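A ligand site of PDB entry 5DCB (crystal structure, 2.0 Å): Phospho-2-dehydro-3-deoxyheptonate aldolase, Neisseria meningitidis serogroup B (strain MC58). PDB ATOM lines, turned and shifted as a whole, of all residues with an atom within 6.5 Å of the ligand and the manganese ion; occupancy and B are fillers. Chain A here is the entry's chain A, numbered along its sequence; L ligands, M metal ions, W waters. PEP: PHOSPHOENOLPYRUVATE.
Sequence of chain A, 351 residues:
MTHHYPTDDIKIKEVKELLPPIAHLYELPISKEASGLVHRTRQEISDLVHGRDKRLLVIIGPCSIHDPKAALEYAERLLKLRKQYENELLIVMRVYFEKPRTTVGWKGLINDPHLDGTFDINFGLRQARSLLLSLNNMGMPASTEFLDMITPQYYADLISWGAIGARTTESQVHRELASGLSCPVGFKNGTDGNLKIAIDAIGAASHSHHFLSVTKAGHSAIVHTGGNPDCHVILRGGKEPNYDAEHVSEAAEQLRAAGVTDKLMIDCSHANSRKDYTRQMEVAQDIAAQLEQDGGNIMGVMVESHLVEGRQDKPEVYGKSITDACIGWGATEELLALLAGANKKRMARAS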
ATOM      1  N   PRO A  62      34.297   4.259  -0.267  1.00  0.00           N
ATOM      2  CA  PRO A  62      34.701   3.715   1.014  1.00  0.00           C
ATOM      3  C   PRO A  62      33.809   2.572   1.507  1.00  0.00           C
ATOM      4  O   PRO A  62      32.643   2.478   1.135  1.00  0.00           O
ATOM      5  CB  PRO A  62      34.558   4.908   1.951  1.00  0.00           C
ATOM      6  CG  PRO A  62      34.785   6.109   1.091  1.00  0.00           C
ATOM      7  CD  PRO A  62      34.287   5.729  -0.275  1.00  0.00           C
ATOM      8  N   CYS A  63      34.362   1.711   2.351  1.00  0.00           N
ATOM      9  CA  CYS A  63      33.546   0.705   2.983  1.00  0.00           C
ATOM     10  C   CYS A  63      32.394   1.379   3.710  1.00  0.00           C
ATOM     11  O   CYS A  63      31.245   0.986   3.568  1.00  0.00           O
ATOM     12  CB  CYS A  63      34.378  -0.116   3.959  1.00  0.00           C
ATOM     13  SG  CYS A  63      33.403  -1.230   5.011  1.00  0.00           S
ATOM     14  N   SER A  64      32.729   2.434   4.457  1.00  0.00           N
ATOM     15  CA  SER A  64      31.777   3.223   5.194  1.00  0.00           C
ATOM     16  C   SER A  64      32.240   4.661   5.213  1.00  0.00           C
ATOM     17  O   SER A  64      33.458   4.937   5.148  1.00  0.00           O
ATOM     18  CB  SER A  64      31.620   2.701   6.624  1.00  0.00           C
ATOM     19  OG  SER A  64      32.813   2.872   7.388  1.00  0.00           O
ATOM     20  N   ARG A  94      30.099   4.780  -3.859  1.00  0.00           N
ATOM     21  CA  ARG A  94      29.633   4.008  -2.722  1.00  0.00           C
ATOM     22  C   ARG A  94      29.545   4.925  -1.506  1.00  0.00           C
ATOM     23  O   ARG A  94      30.566   5.400  -1.032  1.00  0.00           O
ATOM     24  CB  ARG A  94      30.641   2.892  -2.454  1.00  0.00           C
ATOM     25  CG  ARG A  94      30.195   1.848  -1.461  1.00  0.00           C
ATOM     26  CD  ARG A  94      31.230   0.726  -1.274  1.00  0.00           C
ATOM     27  NE  ARG A  94      31.115   0.241   0.082  1.00  0.00           N
ATOM     28  CZ  ARG A  94      30.513  -0.882   0.469  1.00  0.00           C
ATOM     29  NH1 ARG A  94      30.018  -1.735  -0.423  1.00  0.00           N
ATOM     30  NH2 ARG A  94      30.446  -1.154   1.772  1.00  0.00           N
ATOM     31  N   TYR A  96      28.032   4.340   1.887  1.00  0.00           N
ATOM     32  CA  TYR A  96      27.433   3.520   2.933  1.00  0.00           C
ATOM     33  C   TYR A  96      27.804   4.146   4.260  1.00  0.00           C
ATOM     34  O   TYR A  96      28.975   4.376   4.507  1.00  0.00           O
ATOM     35  CB  TYR A  96      27.951   2.074   2.887  1.00  0.00           C
ATOM     36  CG  TYR A  96      27.489   1.266   1.683  1.00  0.00           C
ATOM     37  CD1 TYR A  96      27.233   1.862   0.462  1.00  0.00           C
ATOM     38  CD2 TYR A  96      27.356  -0.113   1.772  1.00  0.00           C
ATOM     39  CE1 TYR A  96      26.824   1.103  -0.647  1.00  0.00           C
ATOM     40  CE2 TYR A  96      26.967  -0.860   0.670  1.00  0.00           C
ATOM     41  CZ  TYR A  96      26.693  -0.255  -0.523  1.00  0.00           C
ATOM     42  OH  TYR A  96      26.334  -1.011  -1.619  1.00  0.00           O
ATOM     43  N   GLU A  98      27.106   2.828   7.321  1.00  0.00           N
ATOM     44  CA  GLU A  98      27.256   1.882   8.413  1.00  0.00           C
ATOM     45  C   GLU A  98      27.709   0.533   7.897  1.00  0.00           C
ATOM     46  O   GLU A  98      27.301   0.103   6.816  1.00  0.00           O
ATOM     47  CB  GLU A  98      25.922   1.721   9.152  1.00  0.00           C
ATOM     48  CG  GLU A  98      25.997   0.759  10.339  1.00  0.00           C
ATOM     49  CD  GLU A  98      24.663   0.554  11.062  1.00  0.00           C
ATOM     50  OE1 GLU A  98      24.607  -0.319  11.979  1.00  0.00           O
ATOM     51  OE2 GLU A  98      23.690   1.281  10.760  1.00  0.00           O
ATOM     52  N   LYS A  99      28.523  -0.166   8.677  1.00  0.00           N
ATOM     53  CA  LYS A  99      28.762  -1.555   8.378  1.00  0.00           C
ATOM     54  C   LYS A  99      28.119  -2.379   9.464  1.00  0.00           C
ATOM     55  O   LYS A  99      28.466  -2.247  10.639  1.00  0.00           O
ATOM     56  CB  LYS A  99      30.237  -1.852   8.295  1.00  0.00           C
ATOM     57  CG  LYS A  99      30.524  -3.182   7.637  1.00  0.00           C
ATOM     58  CD  LYS A  99      31.721  -3.806   8.309  1.00  0.00           C
ATOM     59  CE  LYS A  99      32.403  -4.833   7.440  1.00  0.00           C
ATOM     60  NZ  LYS A  99      31.553  -5.907   6.884  1.00  0.00           N
ATOM     61  N   PRO A 100      27.175  -3.229   9.083  1.00  0.00           N
ATOM     62  CA  PRO A 100      26.572  -4.139  10.033  1.00  0.00           C
ATOM     63  C   PRO A 100      27.661  -4.978  10.667  1.00  0.00           C
ATOM     64  O   PRO A 100      28.649  -5.335   9.999  1.00  0.00           O
ATOM     65  CB  PRO A 100      25.681  -5.026   9.157  1.00  0.00           C
ATOM     66  CG  PRO A 100      25.390  -4.218   7.962  1.00  0.00           C
ATOM     67  CD  PRO A 100      26.597  -3.377   7.730  1.00  0.00           C
ATOM     68  N   GLU A 145      23.436   1.274   1.025  1.00  0.00           N
ATOM     69  CA  GLU A 145      22.701   0.092   1.473  1.00  0.00           C
ATOM     70  C   GLU A 145      21.610   0.517   2.448  1.00  0.00           C
ATOM     71  O   GLU A 145      21.856   1.299   3.340  1.00  0.00           O
ATOM     72  CB  GLU A 145      23.633  -0.880   2.161  1.00  0.00           C
ATOM     73  CG  GLU A 145      22.945  -2.144   2.602  1.00  0.00           C
ATOM     74  CD  GLU A 145      23.940  -3.266   2.859  1.00  0.00           C
ATOM     75  OE1 GLU A 145      24.657  -3.730   1.904  1.00  0.00           O
ATOM     76  OE2 GLU A 145      23.988  -3.657   4.037  1.00  0.00           O
ATOM     77  N   ALA A 163      21.470  -1.045  -2.247  1.00  0.00           N
ATOM     78  CA  ALA A 163      21.855  -2.423  -1.978  1.00  0.00           C
ATOM     79  C   ALA A 163      21.085  -2.951  -0.800  1.00  0.00           C
ATOM     80  O   ALA A 163      20.722  -2.220   0.124  1.00  0.00           O
ATOM     81  CB  ALA A 163      23.336  -2.527  -1.694  1.00  0.00           C
ATOM     82  N   ILE A 164      20.848  -4.241  -0.851  1.00  0.00           N
ATOM     83  CA  ILE A 164      20.415  -4.998   0.295  1.00  0.00           C
ATOM     84  C   ILE A 164      21.494  -6.046   0.545  1.00  0.00           C
ATOM     85  O   ILE A 164      21.788  -6.885  -0.304  1.00  0.00           O
ATOM     86  CB  ILE A 164      19.069  -5.650   0.025  1.00  0.00           C
ATOM     87  CG1 ILE A 164      17.997  -4.598  -0.236  1.00  0.00           C
ATOM     88  CG2 ILE A 164      18.648  -6.563   1.177  1.00  0.00           C
ATOM     89  CD1 ILE A 164      17.661  -3.683   0.945  1.00  0.00           C
ATOM     90  N   GLY A 165      22.093  -5.990   1.730  1.00  0.00           N
ATOM     91  CA  GLY A 165      23.234  -6.827   2.058  1.00  0.00           C
ATOM     92  C   GLY A 165      22.960  -8.293   2.315  1.00  0.00           C
ATOM     93  O   GLY A 165      21.793  -8.735   2.467  1.00  0.00           O
ATOM     94  N   ALA A 166      24.045  -9.065   2.367  1.00  0.00           N
ATOM     95  CA  ALA A 166      24.003 -10.518   2.514  1.00  0.00           C
ATOM     96  C   ALA A 166      23.123 -10.967   3.694  1.00  0.00           C
ATOM     97  O   ALA A 166      22.421 -11.942   3.597  1.00  0.00           O
ATOM     98  CB  ALA A 166      25.427 -11.041   2.711  1.00  0.00           C
ATOM     99  N   LYS A 188      22.734  -8.893  -2.466  1.00  0.00           N
ATOM    100  CA  LYS A 188      23.903  -9.738  -2.228  1.00  0.00           C
ATOM    101  C   LYS A 188      23.545 -11.180  -1.946  1.00  0.00           C
ATOM    102  O   LYS A 188      22.532 -11.465  -1.300  1.00  0.00           O
ATOM    103  CB  LYS A 188      24.753  -9.155  -1.083  1.00  0.00           C
ATOM    104  CG  LYS A 188      25.310  -7.798  -1.443  1.00  0.00           C
ATOM    105  CD  LYS A 188      26.564  -7.426  -0.683  1.00  0.00           C
ATOM    106  CE  LYS A 188      27.603  -6.824  -1.603  1.00  0.00           C
ATOM    107  NZ  LYS A 188      28.862  -6.660  -0.851  1.00  0.00           N
ATOM    108  N   ASN A 189      24.367 -12.105  -2.464  1.00  0.00           N
ATOM    109  CA  ASN A 189      24.254 -13.498  -2.078  1.00  0.00           C
ATOM    110  C   ASN A 189      24.551 -13.613  -0.603  1.00  0.00           C
ATOM    111  O   ASN A 189      25.088 -12.688   0.009  1.00  0.00           O
ATOM    112  CB  ASN A 189      25.111 -14.436  -2.962  1.00  0.00           C
ATOM    113  CG  ASN A 189      26.613 -14.245  -2.806  1.00  0.00           C
ATOM    114  OD1 ASN A 189      27.290 -13.766  -3.729  1.00  0.00           O
ATOM    115  ND2 ASN A 189      27.144 -14.655  -1.670  1.00  0.00           N
ATOM    116  N   THR A 191      25.927 -14.880   3.173  1.00  0.00           N
ATOM    117  CA  THR A 191      27.214 -14.854   3.850  1.00  0.00           C
ATOM    118  C   THR A 191      28.123 -16.021   3.452  1.00  0.00           C
ATOM    119  O   THR A 191      29.325 -15.832   3.225  1.00  0.00           O
ATOM    120  CB  THR A 191      27.015 -14.899   5.367  1.00  0.00           C
ATOM    121  OG1 THR A 191      26.344 -13.709   5.802  1.00  0.00           O
ATOM    122  CG2 THR A 191      28.374 -15.025   6.108  1.00  0.00           C
ATOM    123  N   ARG A 236      29.281 -11.725  -4.057  1.00  0.00           N
ATOM    124  CA  ARG A 236      30.237 -11.236  -3.070  1.00  0.00           C
ATOM    125  C   ARG A 236      31.001 -12.322  -2.335  1.00  0.00           C
ATOM    126  O   ARG A 236      31.634 -12.061  -1.318  1.00  0.00           O
ATOM    127  CB  ARG A 236      29.563 -10.282  -2.056  1.00  0.00           C
ATOM    128  CG  ARG A 236      28.266 -10.747  -1.426  1.00  0.00           C
ATOM    129  CD  ARG A 236      28.465 -11.803  -0.341  1.00  0.00           C
ATOM    130  NE  ARG A 236      29.162 -11.269   0.838  1.00  0.00           N
ATOM    131  CZ  ARG A 236      29.777 -12.030   1.749  1.00  0.00           C
ATOM    132  NH1 ARG A 236      30.377 -11.456   2.775  1.00  0.00           N
ATOM    133  NH2 ARG A 236      29.793 -13.377   1.638  1.00  0.00           N
ATOM    134  N   ASP A 267      31.215  -8.196  -6.696  1.00  0.00           N
ATOM    135  CA  ASP A 267      31.961  -7.458  -5.694  1.00  0.00           C
ATOM    136  C   ASP A 267      33.391  -7.973  -5.638  1.00  0.00           C
ATOM    137  O   ASP A 267      33.609  -9.178  -5.449  1.00  0.00           O
ATOM    138  CB  ASP A 267      31.265  -7.628  -4.353  1.00  0.00           C
ATOM    139  CG  ASP A 267      31.879  -6.809  -3.222  1.00  0.00           C
ATOM    140  OD1 ASP A 267      32.884  -6.078  -3.412  1.00  0.00           O
ATOM    141  OD2 ASP A 267      31.332  -6.915  -2.114  1.00  0.00           O
ATOM    142  N   SER A 269      35.446  -7.060  -3.412  1.00  0.00           N
ATOM    143  CA  SER A 269      35.840  -7.001  -2.023  1.00  0.00           C
ATOM    144  C   SER A 269      35.171  -8.092  -1.153  1.00  0.00           C
ATOM    145  O   SER A 269      34.749  -9.126  -1.659  1.00  0.00           O
ATOM    146  CB  SER A 269      35.544  -5.592  -1.493  1.00  0.00           C
ATOM    147  OG  SER A 269      36.385  -5.323  -0.393  1.00  0.00           O
ATOM    148  N   HIS A 270      35.133  -7.850   0.157  1.00  0.00           N
ATOM    149  CA  HIS A 270      34.522  -8.760   1.127  1.00  0.00           C
ATOM    150  C   HIS A 270      34.957 -10.219   0.928  1.00  0.00           C
ATOM    151  O   HIS A 270      36.149 -10.462   0.806  1.00  0.00           O
ATOM    152  CB  HIS A 270      33.003  -8.540   1.139  1.00  0.00           C
ATOM    153  CG  HIS A 270      32.633  -7.108   1.387  1.00  0.00           C
ATOM    154  ND1 HIS A 270      32.200  -6.273   0.381  1.00  0.00           N
ATOM    155  CD2 HIS A 270      32.699  -6.350   2.505  1.00  0.00           C
ATOM    156  CE1 HIS A 270      31.973  -5.068   0.877  1.00  0.00           C
ATOM    157  NE2 HIS A 270      32.275  -5.083   2.155  1.00  0.00           N
ATOM    158  N   ALA A 271      34.029 -11.177   0.878  1.00  0.00           N
ATOM    159  CA  ALA A 271      34.444 -12.580   0.774  1.00  0.00           C
ATOM    160  C   ALA A 271      35.090 -12.933  -0.572  1.00  0.00           C
ATOM    161  O   ALA A 271      35.764 -13.941  -0.689  1.00  0.00           O
ATOM    162  CB  ALA A 271      33.279 -13.512   1.097  1.00  0.00           C
ATOM    163  N   MET A 302      31.695  -4.061  -7.864  1.00  0.00           N
ATOM    164  CA  MET A 302      31.792  -3.260  -6.641  1.00  0.00           C
ATOM    165  C   MET A 302      33.212  -3.269  -6.109  1.00  0.00           C
ATOM    166  O   MET A 302      33.874  -4.312  -6.053  1.00  0.00           O
ATOM    167  CB  MET A 302      30.846  -3.810  -5.591  1.00  0.00           C
ATOM    168  CG  MET A 302      30.847  -3.012  -4.290  1.00  0.00           C
ATOM    169  SD  MET A 302      29.629  -3.711  -3.159  1.00  0.00           S
ATOM    170  CE  MET A 302      28.119  -3.148  -3.947  1.00  0.00           C
ATOM    171  N   GLU A 304      35.886  -1.538  -2.977  1.00  0.00           N
ATOM    172  CA  GLU A 304      36.050  -0.771  -1.723  1.00  0.00           C
ATOM    173  C   GLU A 304      37.345  -0.013  -1.797  1.00  0.00           C
ATOM    174  O   GLU A 304      38.423  -0.592  -1.796  1.00  0.00           O
ATOM    175  CB  GLU A 304      35.985  -1.656  -0.492  1.00  0.00           C
ATOM    176  CG  GLU A 304      34.597  -2.200  -0.228  1.00  0.00           C
ATOM    177  CD  GLU A 304      34.453  -2.859   1.136  1.00  0.00           C
ATOM    178  OE1 GLU A 304      35.214  -3.834   1.444  1.00  0.00           O
ATOM    179  OE2 GLU A 304      33.556  -2.405   1.895  1.00  0.00           O
ATOM    180  N   THR A 323      36.425   0.837   8.954  1.00  0.00           N
ATOM    181  CA  THR A 323      35.743  -0.455   8.838  1.00  0.00           C
ATOM    182  C   THR A 323      36.593  -1.372   7.913  1.00  0.00           C
ATOM    183  O   THR A 323      37.772  -1.577   8.215  1.00  0.00           O
ATOM    184  CB  THR A 323      34.287  -0.248   8.378  1.00  0.00           C
ATOM    185  OG1 THR A 323      34.265   0.611   7.224  1.00  0.00           O
ATOM    186  CG2 THR A 323      33.482   0.400   9.482  1.00  0.00           C
ATOM    187  N   ASP A 324      36.062  -1.892   6.809  1.00  0.00           N
ATOM    188  CA  ASP A 324      36.830  -2.824   5.967  1.00  0.00           C
ATOM    189  C   ASP A 324      37.951  -2.057   5.262  1.00  0.00           C
ATOM    190  O   ASP A 324      37.780  -0.898   4.859  1.00  0.00           O
ATOM    191  CB  ASP A 324      35.951  -3.483   4.890  1.00  0.00           C
ATOM    192  CG  ASP A 324      34.883  -4.388   5.459  1.00  0.00           C
ATOM    193  OD1 ASP A 324      35.083  -4.934   6.549  1.00  0.00           O
ATOM    194  OD2 ASP A 324      33.823  -4.548   4.844  1.00  0.00           O
ATOM    195  N   ALA A 325      39.105  -2.718   5.108  1.00  0.00           N
ATOM    196  CA  ALA A 325      40.255  -2.141   4.433  1.00  0.00           C
ATOM    197  C   ALA A 325      39.953  -1.925   2.963  1.00  0.00           C
ATOM    198  O   ALA A 325      39.347  -2.746   2.327  1.00  0.00           O
ATOM    199  CB  ALA A 325      41.480  -3.056   4.595  1.00  0.00           C
HETATM  200  C1  PEP L   1      29.544  -8.135   2.525  1.00  0.00           C
HETATM  201  O1  PEP L   1      29.371  -8.461   1.332  1.00  0.00           O
HETATM  202  O2' PEP L   1      29.906  -8.965   3.382  1.00  0.00           O
HETATM  203  C2  PEP L   1      29.341  -6.736   2.919  1.00  0.00           C
HETATM  204  C3  PEP L   1      29.270  -6.391   4.209  1.00  0.00           C
HETATM  205  O2  PEP L   1      29.241  -5.782   1.818  1.00  0.00           O
HETATM  206  P   PEP L   1      28.341  -4.455   1.815  1.00  0.00           P
HETATM  207  O1P PEP L   1      28.481  -4.016   0.372  1.00  0.00           O
HETATM  208  O2P PEP L   1      26.973  -4.984   2.194  1.00  0.00           O
HETATM  209  O3P PEP L   1      29.046  -3.554   2.796  1.00  0.00           O
HETATM  210 MN    MN M   1      32.912  -3.304   3.565  1.00  0.00          MN
HETATM  211  O   HOH W   1      30.927  -3.251   4.244  1.00  0.00           O
HETATM  212  O   HOH W   2      26.423  -7.481   2.911  1.00  0.00           O
HETATM  213  O   HOH W   3      27.410  -2.430   4.700  1.00  0.00           O
HETATM  214  O   HOH W   4      26.248  -3.766  -0.985  1.00  0.00           O
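The manganese ion is bound by the side-chain carboxylate (OE2) of Glu 304, the side-chain carboxylate (OD2) of Asp 324, water W1, a ring nitrogen (NE2) of His 270 and the side-chain sulfur (SG) of Cys 63.
ND1 of His 270 lies close to O2 of the ligand, at 3.3 Å.
The guanidinium group of Arg 236 lies within salt-bridge range of an oxygen (O2') of the ligand (2.6 Å).
OE1 of Glu 145 sits close to O2P of the ligand, at 2.6 Å.
NZ of Lys 188 is in salt-bridge range of O1 of the ligand (2.9 Å).
NH1 of Arg 94 lies within salt-bridge range of O1P of the ligand (2.9 Å).
Water W4 lies within hydrogen-bond range of an oxygen (O1P) of the ligand, the side-chain hydroxyl of Tyr 96 and the side-chain carboxylate of Glu 145.
Water W2 bridges O2P of the ligand (2.7 Å) and N of Ala 166 (2.9 Å).
Water W3 lies within hydrogen-bond range of O3P of the ligand (2.8 Å) and O of Glu 98 (3.3 Å).
The side-chain sulfur of Met 302 lies close to an oxygen (O1P) of the ligand (3.7 Å).
Residues that only touch the ligand: Tyr 96 (3.5 Å) and Lys 99 (3.5 Å).
Hydrophobic or aromatic side chains that line the ligand: Tyr 96, His 270 and Met 302.
Within 4 Å of the ligand: Arg 94, Tyr 96, Lys 99, Glu 145, Lys 188, Arg 236, His 270 and Met 302.
NH2 of Arg 94 touches the manganese ion (3.7 Å).
Of the 26 residues printed, 5 come within 4 Å of the manganese ion.
OE2 of Glu 304 sits close to NH2 of Arg 94.
The side-chain carboxylate (OD1) of Asp 324 is in salt-bridge range of the side-chain amino group (NZ) of Lys 99 (3.7 Å).
ND1 of His 270 is in hydrogen-bond range of OD2 of Asp 267, 2.7 Å away.
The backbone carbonyl oxygen of Cys 63 sits at hydrogen-bond distance from the guanidinium group of Arg 94 (2.9 Å).
The side-chain sulfur (SG) of Cys 63 lies close to the side-chain hydroxyl (OG1) of Thr 323 (3.0 Å).
The guanidinium group (NH2) of Arg 236 lies within hydrogen-bond range of the backbone carbonyl oxygen (O) of Thr 191 (3.0 Å).
O of Ile 164 lies within hydrogen-bond range of N of Lys 188.
The backbone carbonyl oxygen (O) of Pro 62 sits at hydrogen-bond distance from the guanidinium group (NE) of Arg 94, at 2.9 Å.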
